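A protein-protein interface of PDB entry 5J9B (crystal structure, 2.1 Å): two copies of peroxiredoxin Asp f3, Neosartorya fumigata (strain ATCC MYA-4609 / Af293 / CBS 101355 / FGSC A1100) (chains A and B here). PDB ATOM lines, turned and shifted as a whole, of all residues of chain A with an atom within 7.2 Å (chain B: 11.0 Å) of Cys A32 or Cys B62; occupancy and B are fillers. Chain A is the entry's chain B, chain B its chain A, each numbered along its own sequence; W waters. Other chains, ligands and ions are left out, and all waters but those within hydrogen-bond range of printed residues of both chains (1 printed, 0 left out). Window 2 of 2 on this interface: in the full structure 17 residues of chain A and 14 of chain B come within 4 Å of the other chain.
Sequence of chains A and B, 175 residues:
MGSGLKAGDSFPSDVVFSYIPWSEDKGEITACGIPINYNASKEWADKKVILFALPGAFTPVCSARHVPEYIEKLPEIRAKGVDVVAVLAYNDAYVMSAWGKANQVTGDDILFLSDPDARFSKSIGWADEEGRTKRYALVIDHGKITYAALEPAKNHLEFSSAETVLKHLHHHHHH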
ATOM      1  N   ILE A  20      33.318  11.290 -28.660  1.00  0.00           N
ATOM      2  CA  ILE A  20      32.145  11.949 -28.106  1.00  0.00           C
ATOM      3  C   ILE A  20      32.593  12.927 -27.039  1.00  0.00           C
ATOM      4  O   ILE A  20      33.142  12.500 -26.030  1.00  0.00           O
ATOM      5  CB  ILE A  20      31.170  10.948 -27.465  1.00  0.00           C
ATOM      6  CG1 ILE A  20      30.717   9.916 -28.491  1.00  0.00           C
ATOM      7  CG2 ILE A  20      29.977  11.676 -26.838  1.00  0.00           C
ATOM      8  CD1 ILE A  20      29.763   8.927 -27.914  1.00  0.00           C
ATOM      9  N   GLU A  24      27.008  15.682 -19.467  1.00  0.00           N
ATOM     10  CA  GLU A  24      25.801  14.979 -18.999  1.00  0.00           C
ATOM     11  C   GLU A  24      25.938  14.118 -17.746  1.00  0.00           C
ATOM     12  O   GLU A  24      26.869  14.281 -16.954  1.00  0.00           O
ATOM     13  CB  GLU A  24      25.237  14.113 -20.134  1.00  0.00           C
ATOM     14  CG  GLU A  24      24.528  14.928 -21.208  1.00  0.00           C
ATOM     15  CD  GLU A  24      24.410  14.188 -22.526  1.00  0.00           C
ATOM     16  OE1 GLU A  24      24.906  13.039 -22.603  1.00  0.00           O
ATOM     17  OE2 GLU A  24      23.824  14.757 -23.481  1.00  0.00           O
ATOM     18  N   ILE A  29      26.800   5.409 -19.654  1.00  0.00           N
ATOM     19  CA  ILE A  29      25.968   5.422 -20.845  1.00  0.00           C
ATOM     20  C   ILE A  29      25.754   6.833 -21.401  1.00  0.00           C
ATOM     21  O   ILE A  29      25.175   7.691 -20.730  1.00  0.00           O
ATOM     22  CB  ILE A  29      24.615   4.764 -20.541  1.00  0.00           C
ATOM     23  CG1 ILE A  29      24.058   5.306 -19.216  1.00  0.00           C
ATOM     24  CG2 ILE A  29      24.785   3.246 -20.481  1.00  0.00           C
ATOM     25  CD1 ILE A  29      22.792   4.624 -18.727  1.00  0.00           C
ATOM     26  N   THR A  30      26.237   7.080 -22.619  1.00  0.00           N
ATOM     27  CA  THR A  30      26.000   8.375 -23.254  1.00  0.00           C
ATOM     28  C   THR A  30      24.522   8.467 -23.591  1.00  0.00           C
ATOM     29  O   THR A  30      23.958   7.549 -24.194  1.00  0.00           O
ATOM     30  CB  THR A  30      26.850   8.604 -24.536  1.00  0.00           C
ATOM     31  OG1 THR A  30      26.442   7.705 -25.575  1.00  0.00           O
ATOM     32  CG2 THR A  30      28.330   8.425 -24.252  1.00  0.00           C
ATOM     33  N   ALA A  31      23.897   9.560 -23.166  1.00  0.00           N
ATOM     34  CA  ALA A  31      22.475   9.766 -23.370  1.00  0.00           C
ATOM     35  C   ALA A  31      22.125   9.614 -24.841  1.00  0.00           C
ATOM     36  O   ALA A  31      21.260   8.822 -25.214  1.00  0.00           O
ATOM     37  CB  ALA A  31      22.058  11.148 -22.857  1.00  0.00           C
ATOM     38  N   CYS A  32      22.832  10.357 -25.676  1.00  0.00           N
ATOM     39  CA  CYS A  32      22.532  10.401 -27.092  1.00  0.00           C
ATOM     40  C   CYS A  32      23.705  11.064 -27.778  1.00  0.00           C
ATOM     41  O   CYS A  32      23.552  11.734 -28.813  1.00  0.00           O
ATOM     42  CB  CYS A  32      21.229  11.163 -27.359  1.00  0.00           C
ATOM     43  SG  CYS A  32      20.333  10.664 -28.856  1.00  0.00           S
ATOM     44  N   GLY A  33      24.881  10.876 -27.182  1.00  0.00           N
ATOM     45  CA  GLY A  33      26.109  11.405 -27.739  1.00  0.00           C
ATOM     46  C   GLY A  33      26.300  10.845 -29.130  1.00  0.00           C
ATOM     47  O   GLY A  33      25.892   9.718 -29.410  1.00  0.00           O
ATOM     48  N   ILE A  34      26.889  11.637 -30.015  1.00  0.00           N
ATOM     49  CA  ILE A  34      27.096  11.194 -31.386  1.00  0.00           C
ATOM     50  C   ILE A  34      28.544  11.467 -31.797  1.00  0.00           C
ATOM     51  O   ILE A  34      29.073  12.549 -31.548  1.00  0.00           O
ATOM     52  CB  ILE A  34      26.098  11.873 -32.341  1.00  0.00           C
ATOM     53  CG1 ILE A  34      26.360  11.456 -33.796  1.00  0.00           C
ATOM     54  CG2 ILE A  34      26.120  13.397 -32.158  1.00  0.00           C
ATOM     55  CD1 ILE A  34      25.152  11.607 -34.713  1.00  0.00           C
ATOM     56  N   PRO A  35      29.206  10.459 -32.384  1.00  0.00           N
ATOM     57  CA  PRO A  35      30.622  10.566 -32.746  1.00  0.00           C
ATOM     58  C   PRO A  35      30.885  11.680 -33.737  1.00  0.00           C
ATOM     59  O   PRO A  35      30.277  11.721 -34.802  1.00  0.00           O
ATOM     60  CB  PRO A  35      30.928   9.202 -33.377  1.00  0.00           C
ATOM     61  CG  PRO A  35      29.919   8.289 -32.799  1.00  0.00           C
ATOM     62  CD  PRO A  35      28.678   9.112 -32.659  1.00  0.00           C
ATOM     63  N   TYR A  94      31.690   5.549 -28.887  1.00  0.00           N
ATOM     64  CA  TYR A  94      30.772   5.212 -27.794  1.00  0.00           C
ATOM     65  C   TYR A  94      31.471   4.449 -26.668  1.00  0.00           C
ATOM     66  O   TYR A  94      31.290   4.758 -25.489  1.00  0.00           O
ATOM     67  CB  TYR A  94      29.581   4.390 -28.312  1.00  0.00           C
ATOM     68  CG  TYR A  94      28.691   5.157 -29.280  1.00  0.00           C
ATOM     69  CD1 TYR A  94      28.074   6.335 -28.890  1.00  0.00           C
ATOM     70  CD2 TYR A  94      28.461   4.697 -30.570  1.00  0.00           C
ATOM     71  CE1 TYR A  94      27.272   7.051 -29.759  1.00  0.00           C
ATOM     72  CE2 TYR A  94      27.643   5.408 -31.450  1.00  0.00           C
ATOM     73  CZ  TYR A  94      27.050   6.576 -31.033  1.00  0.00           C
ATOM     74  OH  TYR A  94      26.238   7.284 -31.892  1.00  0.00           O
ATOM     75  N   PHE B  58      27.556  -0.389 -25.792  1.00  0.00           N
ATOM     76  CA  PHE B  58      27.561   1.026 -25.402  1.00  0.00           C
ATOM     77  C   PHE B  58      26.978   2.008 -26.431  1.00  0.00           C
ATOM     78  O   PHE B  58      27.170   3.205 -26.312  1.00  0.00           O
ATOM     79  CB  PHE B  58      28.977   1.457 -25.013  1.00  0.00           C
ATOM     80  CG  PHE B  58      29.429   0.903 -23.684  1.00  0.00           C
ATOM     81  CD1 PHE B  58      28.935   1.422 -22.500  1.00  0.00           C
ATOM     82  CD2 PHE B  58      30.324  -0.144 -23.624  1.00  0.00           C
ATOM     83  CE1 PHE B  58      29.344   0.920 -21.283  1.00  0.00           C
ATOM     84  CE2 PHE B  58      30.735  -0.654 -22.400  1.00  0.00           C
ATOM     85  CZ  PHE B  58      30.244  -0.121 -21.233  1.00  0.00           C
ATOM     86  N   THR B  59      26.237   1.515 -27.414  1.00  0.00           N
ATOM     87  CA  THR B  59      25.406   2.407 -28.233  1.00  0.00           C
ATOM     88  C   THR B  59      24.493   3.235 -27.314  1.00  0.00           C
ATOM     89  O   THR B  59      24.107   2.775 -26.240  1.00  0.00           O
ATOM     90  CB  THR B  59      24.567   1.624 -29.239  1.00  0.00           C
ATOM     91  OG1 THR B  59      23.948   0.529 -28.557  1.00  0.00           O
ATOM     92  CG2 THR B  59      25.454   1.087 -30.354  1.00  0.00           C
ATOM     93  N   PRO B  60      24.163   4.470 -27.715  1.00  0.00           N
ATOM     94  CA  PRO B  60      23.571   5.358 -26.703  1.00  0.00           C
ATOM     95  C   PRO B  60      22.213   4.898 -26.170  1.00  0.00           C
ATOM     96  O   PRO B  60      21.573   4.002 -26.722  1.00  0.00           O
ATOM     97  CB  PRO B  60      23.418   6.701 -27.442  1.00  0.00           C
ATOM     98  CG  PRO B  60      24.158   6.562 -28.718  1.00  0.00           C
ATOM     99  CD  PRO B  60      24.249   5.108 -29.039  1.00  0.00           C
ATOM    100  N   VAL B  61      21.799   5.533 -25.081  1.00  0.00           N
ATOM    101  CA  VAL B  61      20.514   5.281 -24.442  1.00  0.00           C
ATOM    102  C   VAL B  61      19.344   5.657 -25.356  1.00  0.00           C
ATOM    103  O   VAL B  61      18.346   4.944 -25.440  1.00  0.00           O
ATOM    104  CB  VAL B  61      20.414   6.066 -23.115  1.00  0.00           C
ATOM    105  CG1 VAL B  61      19.069   5.845 -22.436  1.00  0.00           C
ATOM    106  CG2 VAL B  61      21.565   5.683 -22.186  1.00  0.00           C
ATOM    107  N   CYS B  62      19.484   6.778 -26.053  1.00  0.00           N
ATOM    108  CA  CYS B  62      18.437   7.265 -26.945  1.00  0.00           C
ATOM    109  C   CYS B  62      18.185   6.369 -28.158  1.00  0.00           C
ATOM    110  O   CYS B  62      17.171   6.503 -28.833  1.00  0.00           O
ATOM    111  CB  CYS B  62      18.795   8.667 -27.422  1.00  0.00           C
ATOM    112  SG  CYS B  62      20.324   8.687 -28.369  1.00  0.00           S
ATOM    113  N   SER B  63      19.114   5.477 -28.468  1.00  0.00           N
ATOM    114  CA  SER B  63      18.912   4.603 -29.619  1.00  0.00           C
ATOM    115  C   SER B  63      18.113   3.371 -29.174  1.00  0.00           C
ATOM    116  O   SER B  63      17.553   3.358 -28.066  1.00  0.00           O
ATOM    117  CB  SER B  63      20.248   4.210 -30.258  1.00  0.00           C
ATOM    118  OG  SER B  63      21.097   3.590 -29.310  1.00  0.00           O
ATOM    119  N   ALA B  64      18.049   2.354 -30.033  1.00  0.00           N
ATOM    120  CA  ALA B  64      17.184   1.196 -29.801  1.00  0.00           C
ATOM    121  C   ALA B  64      17.367   0.586 -28.407  1.00  0.00           C
ATOM    122  O   ALA B  64      18.489   0.304 -27.990  1.00  0.00           O
ATOM    123  CB  ALA B  64      17.430   0.141 -30.872  1.00  0.00           C
ATOM    124  N   ARG B  65      16.258   0.408 -27.693  1.00  0.00           N
ATOM    125  CA  ARG B  65      16.277  -0.214 -26.370  1.00  0.00           C
ATOM    126  C   ARG B  65      16.304  -1.740 -26.445  1.00  0.00           C
ATOM    127  O   ARG B  65      15.418  -2.393 -25.903  1.00  0.00           O
ATOM    128  CB  ARG B  65      15.059   0.225 -25.546  1.00  0.00           C
ATOM    129  CG  ARG B  65      15.083   1.684 -25.116  1.00  0.00           C
ATOM    130  CD  ARG B  65      13.899   2.051 -24.211  1.00  0.00           C
ATOM    131  NE  ARG B  65      14.070   1.539 -22.857  1.00  0.00           N
ATOM    132  CZ  ARG B  65      13.309   0.596 -22.308  1.00  0.00           C
ATOM    133  NH1 ARG B  65      12.299   0.074 -22.993  1.00  0.00           N
ATOM    134  NH2 ARG B  65      13.553   0.180 -21.073  1.00  0.00           N
ATOM    135  N   HIS B  66      17.327  -2.310 -27.081  1.00  0.00           N
ATOM    136  CA  HIS B  66      17.364  -3.762 -27.280  1.00  0.00           C
ATOM    137  C   HIS B  66      17.537  -4.521 -25.960  1.00  0.00           C
ATOM    138  O   HIS B  66      16.676  -5.313 -25.566  1.00  0.00           O
ATOM    139  CB  HIS B  66      18.480  -4.158 -28.260  1.00  0.00           C
ATOM    140  CG  HIS B  66      18.192  -5.420 -29.022  1.00  0.00           C
ATOM    141  ND1 HIS B  66      18.944  -5.831 -30.102  1.00  0.00           N
ATOM    142  CD2 HIS B  66      17.220  -6.353 -28.867  1.00  0.00           C
ATOM    143  CE1 HIS B  66      18.449  -6.960 -30.577  1.00  0.00           C
ATOM    144  NE2 HIS B  66      17.406  -7.303 -29.843  1.00  0.00           N
ATOM    145  N   PRO B  68      17.666  -3.272 -22.705  1.00  0.00           N
ATOM    146  CA  PRO B  68      16.784  -2.983 -21.566  1.00  0.00           C
ATOM    147  C   PRO B  68      15.449  -3.706 -21.658  1.00  0.00           C
ATOM    148  O   PRO B  68      14.951  -4.163 -20.631  1.00  0.00           O
ATOM    149  CB  PRO B  68      16.588  -1.464 -21.645  1.00  0.00           C
ATOM    150  CG  PRO B  68      17.795  -0.967 -22.362  1.00  0.00           C
ATOM    151  CD  PRO B  68      18.101  -2.032 -23.379  1.00  0.00           C
ATOM    152  N   GLU B  69      14.897  -3.830 -22.864  1.00  0.00           N
ATOM    153  CA  GLU B  69      13.666  -4.599 -23.070  1.00  0.00           C
ATOM    154  C   GLU B  69      13.819  -6.071 -22.723  1.00  0.00           C
ATOM    155  O   GLU B  69      12.878  -6.677 -22.214  1.00  0.00           O
ATOM    156  CB  GLU B  69      13.175  -4.475 -24.511  1.00  0.00           C
ATOM    157  CG  GLU B  69      12.604  -3.116 -24.818  1.00  0.00           C
ATOM    158  CD  GLU B  69      12.265  -2.937 -26.283  1.00  0.00           C
ATOM    159  OE1 GLU B  69      12.156  -3.954 -27.011  1.00  0.00           O
ATOM    160  OE2 GLU B  69      12.124  -1.768 -26.699  1.00  0.00           O
ATOM    161  N   TRP B  99      29.820  -3.477 -20.290  1.00  0.00           N
ATOM    162  CA  TRP B  99      28.475  -3.104 -20.752  1.00  0.00           C
ATOM    163  C   TRP B  99      27.372  -3.769 -19.936  1.00  0.00           C
ATOM    164  O   TRP B  99      26.308  -3.195 -19.715  1.00  0.00           O
ATOM    165  CB  TRP B  99      28.287  -3.472 -22.222  1.00  0.00           C
ATOM    166  CG  TRP B  99      27.117  -2.795 -22.878  1.00  0.00           C
ATOM    167  CD1 TRP B  99      26.636  -1.530 -22.623  1.00  0.00           C
ATOM    168  CD2 TRP B  99      26.296  -3.332 -23.926  1.00  0.00           C
ATOM    169  NE1 TRP B  99      25.564  -1.258 -23.450  1.00  0.00           N
ATOM    170  CE2 TRP B  99      25.333  -2.350 -24.252  1.00  0.00           C
ATOM    171  CE3 TRP B  99      26.283  -4.548 -24.616  1.00  0.00           C
ATOM    172  CZ2 TRP B  99      24.364  -2.557 -25.236  1.00  0.00           C
ATOM    173  CZ3 TRP B  99      25.320  -4.751 -25.598  1.00  0.00           C
ATOM    174  CH2 TRP B  99      24.374  -3.763 -25.894  1.00  0.00           C
ATOM    175  N   ASN B 103      24.568  -1.937 -17.665  1.00  0.00           N
ATOM    176  CA  ASN B 103      23.132  -2.205 -17.761  1.00  0.00           C
ATOM    177  C   ASN B 103      22.589  -2.811 -16.473  1.00  0.00           C
ATOM    178  O   ASN B 103      21.447  -3.274 -16.434  1.00  0.00           O
ATOM    179  CB  ASN B 103      22.821  -3.137 -18.937  1.00  0.00           C
ATOM    180  CG  ASN B 103      22.926  -2.441 -20.288  1.00  0.00           C
ATOM    181  OD1 ASN B 103      21.984  -1.779 -20.735  1.00  0.00           O
ATOM    182  ND2 ASN B 103      24.076  -2.595 -20.948  1.00  0.00           N
ATOM    183  N   ARG B 135      21.966  -6.986 -36.284  1.00  0.00           N
ATOM    184  CA  ARG B 135      20.989  -7.145 -35.226  1.00  0.00           C
ATOM    185  C   ARG B 135      20.059  -8.307 -35.574  1.00  0.00           C
ATOM    186  O   ARG B 135      19.367  -8.276 -36.597  1.00  0.00           O
ATOM    187  CB  ARG B 135      20.185  -5.860 -35.024  1.00  0.00           C
ATOM    188  CG  ARG B 135      19.415  -5.841 -33.700  1.00  0.00           C
ATOM    189  CD  ARG B 135      18.595  -4.571 -33.507  1.00  0.00           C
ATOM    190  NE  ARG B 135      19.397  -3.355 -33.610  1.00  0.00           N
ATOM    191  CZ  ARG B 135      19.999  -2.775 -32.578  1.00  0.00           C
ATOM    192  NH1 ARG B 135      19.905  -3.313 -31.357  1.00  0.00           N
ATOM    193  NH2 ARG B 135      20.701  -1.669 -32.762  1.00  0.00           N
ATOM    194  N   ASN B 155      19.522  -0.243 -37.129  1.00  0.00           N
ATOM    195  CA  ASN B 155      18.830   0.287 -35.961  1.00  0.00           C
ATOM    196  C   ASN B 155      17.321   0.042 -35.987  1.00  0.00           C
ATOM    197  O   ASN B 155      16.569   0.683 -35.250  1.00  0.00           O
ATOM    198  CB  ASN B 155      19.135   1.776 -35.828  1.00  0.00           C
ATOM    199  CG  ASN B 155      20.613   2.033 -35.625  1.00  0.00           C
ATOM    200  OD1 ASN B 155      21.260   1.374 -34.797  1.00  0.00           O
ATOM    201  ND2 ASN B 155      21.169   2.963 -36.399  1.00  0.00           N
ATOM    202  N   HIS B 156      16.897  -0.900 -36.831  1.00  0.00           N
ATOM    203  CA  HIS B 156      15.522  -1.389 -36.836  1.00  0.00           C
ATOM    204  C   HIS B 156      15.346  -2.423 -35.735  1.00  0.00           C
ATOM    205  O   HIS B 156      16.026  -3.445 -35.739  1.00  0.00           O
ATOM    206  CB  HIS B 156      15.176  -2.009 -38.191  1.00  0.00           C
ATOM    207  CG  HIS B 156      13.725  -2.340 -38.356  1.00  0.00           C
ATOM    208  ND1 HIS B 156      12.832  -1.490 -38.971  1.00  0.00           N
ATOM    209  CD2 HIS B 156      13.010  -3.430 -37.991  1.00  0.00           C
ATOM    210  CE1 HIS B 156      11.633  -2.040 -38.981  1.00  0.00           C
ATOM    211  NE2 HIS B 156      11.713  -3.219 -38.391  1.00  0.00           N
ATOM    212  N   LEU B 157      14.445  -2.170 -34.792  1.00  0.00           N
ATOM    213  CA  LEU B 157      14.262  -3.091 -33.680  1.00  0.00           C
ATOM    214  C   LEU B 157      12.850  -3.608 -33.698  1.00  0.00           C
ATOM    215  O   LEU B 157      11.905  -2.889 -33.363  1.00  0.00           O
ATOM    216  CB  LEU B 157      14.567  -2.421 -32.337  1.00  0.00           C
ATOM    217  CG  LEU B 157      14.384  -3.242 -31.047  1.00  0.00           C
ATOM    218  CD1 LEU B 157      15.119  -4.587 -31.118  1.00  0.00           C
ATOM    219  CD2 LEU B 157      14.860  -2.442 -29.818  1.00  0.00           C
HETATM  220  O   HOH W   1      28.724   5.328 -24.336  1.00  0.00           O
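The backbone carbonyl oxygen (O) of Thr A30 lies within hydrogen-bond range of the backbone NH (N) of Val B61 (3.1 Å). The backbone carbonyl oxygen (O) of Ala A31 lies within hydrogen-bond range of the backbone NH (N) of Val B61 (3.3 Å). The backbone NH of Cys B62 lies within hydrogen-bond range of the backbone carbonyl oxygen of Ala A31 (2.8 Å). The side-chain sulfur (SG) of Cys B62 forms a disulfide with the side-chain sulfur (SG) of Cys A32 (2.0 Å).
The side-chain hydroxyl (OG) of Ser B63 lies within hydrogen-bond range of the backbone carbonyl oxygen (O) of Pro B60 (2.7 Å). OH of Tyr A94 lies close to O of Gly A33.
Ile A29 touches Val B61 (CB to CG2, 3.6 Å). O of Thr A30 touches CA of Pro B60, at 3.4 Å. Ala A31 touches Pro B60. CA of Cys A32 touches CB of Pro B60 (3.8 Å). O of Gly A33 touches CG of Pro B60, at 3.7 Å. Phe B58 touches Tyr A94 (O to CB, 3.3 Å). CE1 of Tyr A94 touches CG of Pro B60 (3.3 Å).
Printed residues of chain B within 4 Å of Ile A29: Val B61 (3.6 Å). Of chain B, only Pro B60 and Val B61 come within 4 Å of Thr A30. Of the printed residues of chain B, Ala A31 touches Pro B60, Val B61 and Cys B62. Printed residues of chain B within 4 Å of Cys A32: Pro B60 (3.8 Å) and Cys B62 (2.0 Å). Gly A33 touches one residue of chain B. Printed residues of chain B within 4 Å of Tyr A94: Phe B58 and Pro B60. Of the printed residues of chain A, Pro B60 touches Thr A30 (3.4 Å), Ala A31 (3.8 Å), Cys A32 (3.8 Å), Gly A33 (3.7 Å) and Tyr A94 (3.3 Å). Of the printed residues of chain A, Val B61 touches Ile A29, Thr A30 and Ala A31. Cys B62 touches just these residues of chain A: Ala A31 (2.8 Å) and Cys A32 (2.0 Å). Asn B103 touches none of the printed residues of chain A. His B156 touches none of the printed residues of chain A. The nearest residue of chain A that does not touch Cys B62 is Thr A30 (4.9 Å). The nearest printed residue of chain A that does not touch Val B61 is Cys A32 (5.0 Å).
Printed residues of chain B that touch a printed residue of chain A: Phe B58, Pro B60, Val B61 and Cys B62. Hydrophobic or aromatic side chains of chain B that line the printed part of chain A: Pro B60 and Val B61. Along chain B the printed residues that touch a printed residue of chain A span positions 58 to 62. Among the printed residues, 11 pairs touch across the chains. Among the printed residues, no Asp or Glu carboxylate lies within 4 Å of a Lys or Arg side-chain nitrogen of the other chain.
No position is printed for both chains. Of the 11 pairs that touch across the chains among the printed residues, none has its exchanged pair printed and touching as well.
Water W1 lies within hydrogen-bond range of the backbone carbonyl oxygen of Tyr A94 (2.9 Å), the backbone carbonyl oxygen of Phe B58 (3.3 Å) and the backbone NH of Thr A30 (3.5 Å).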
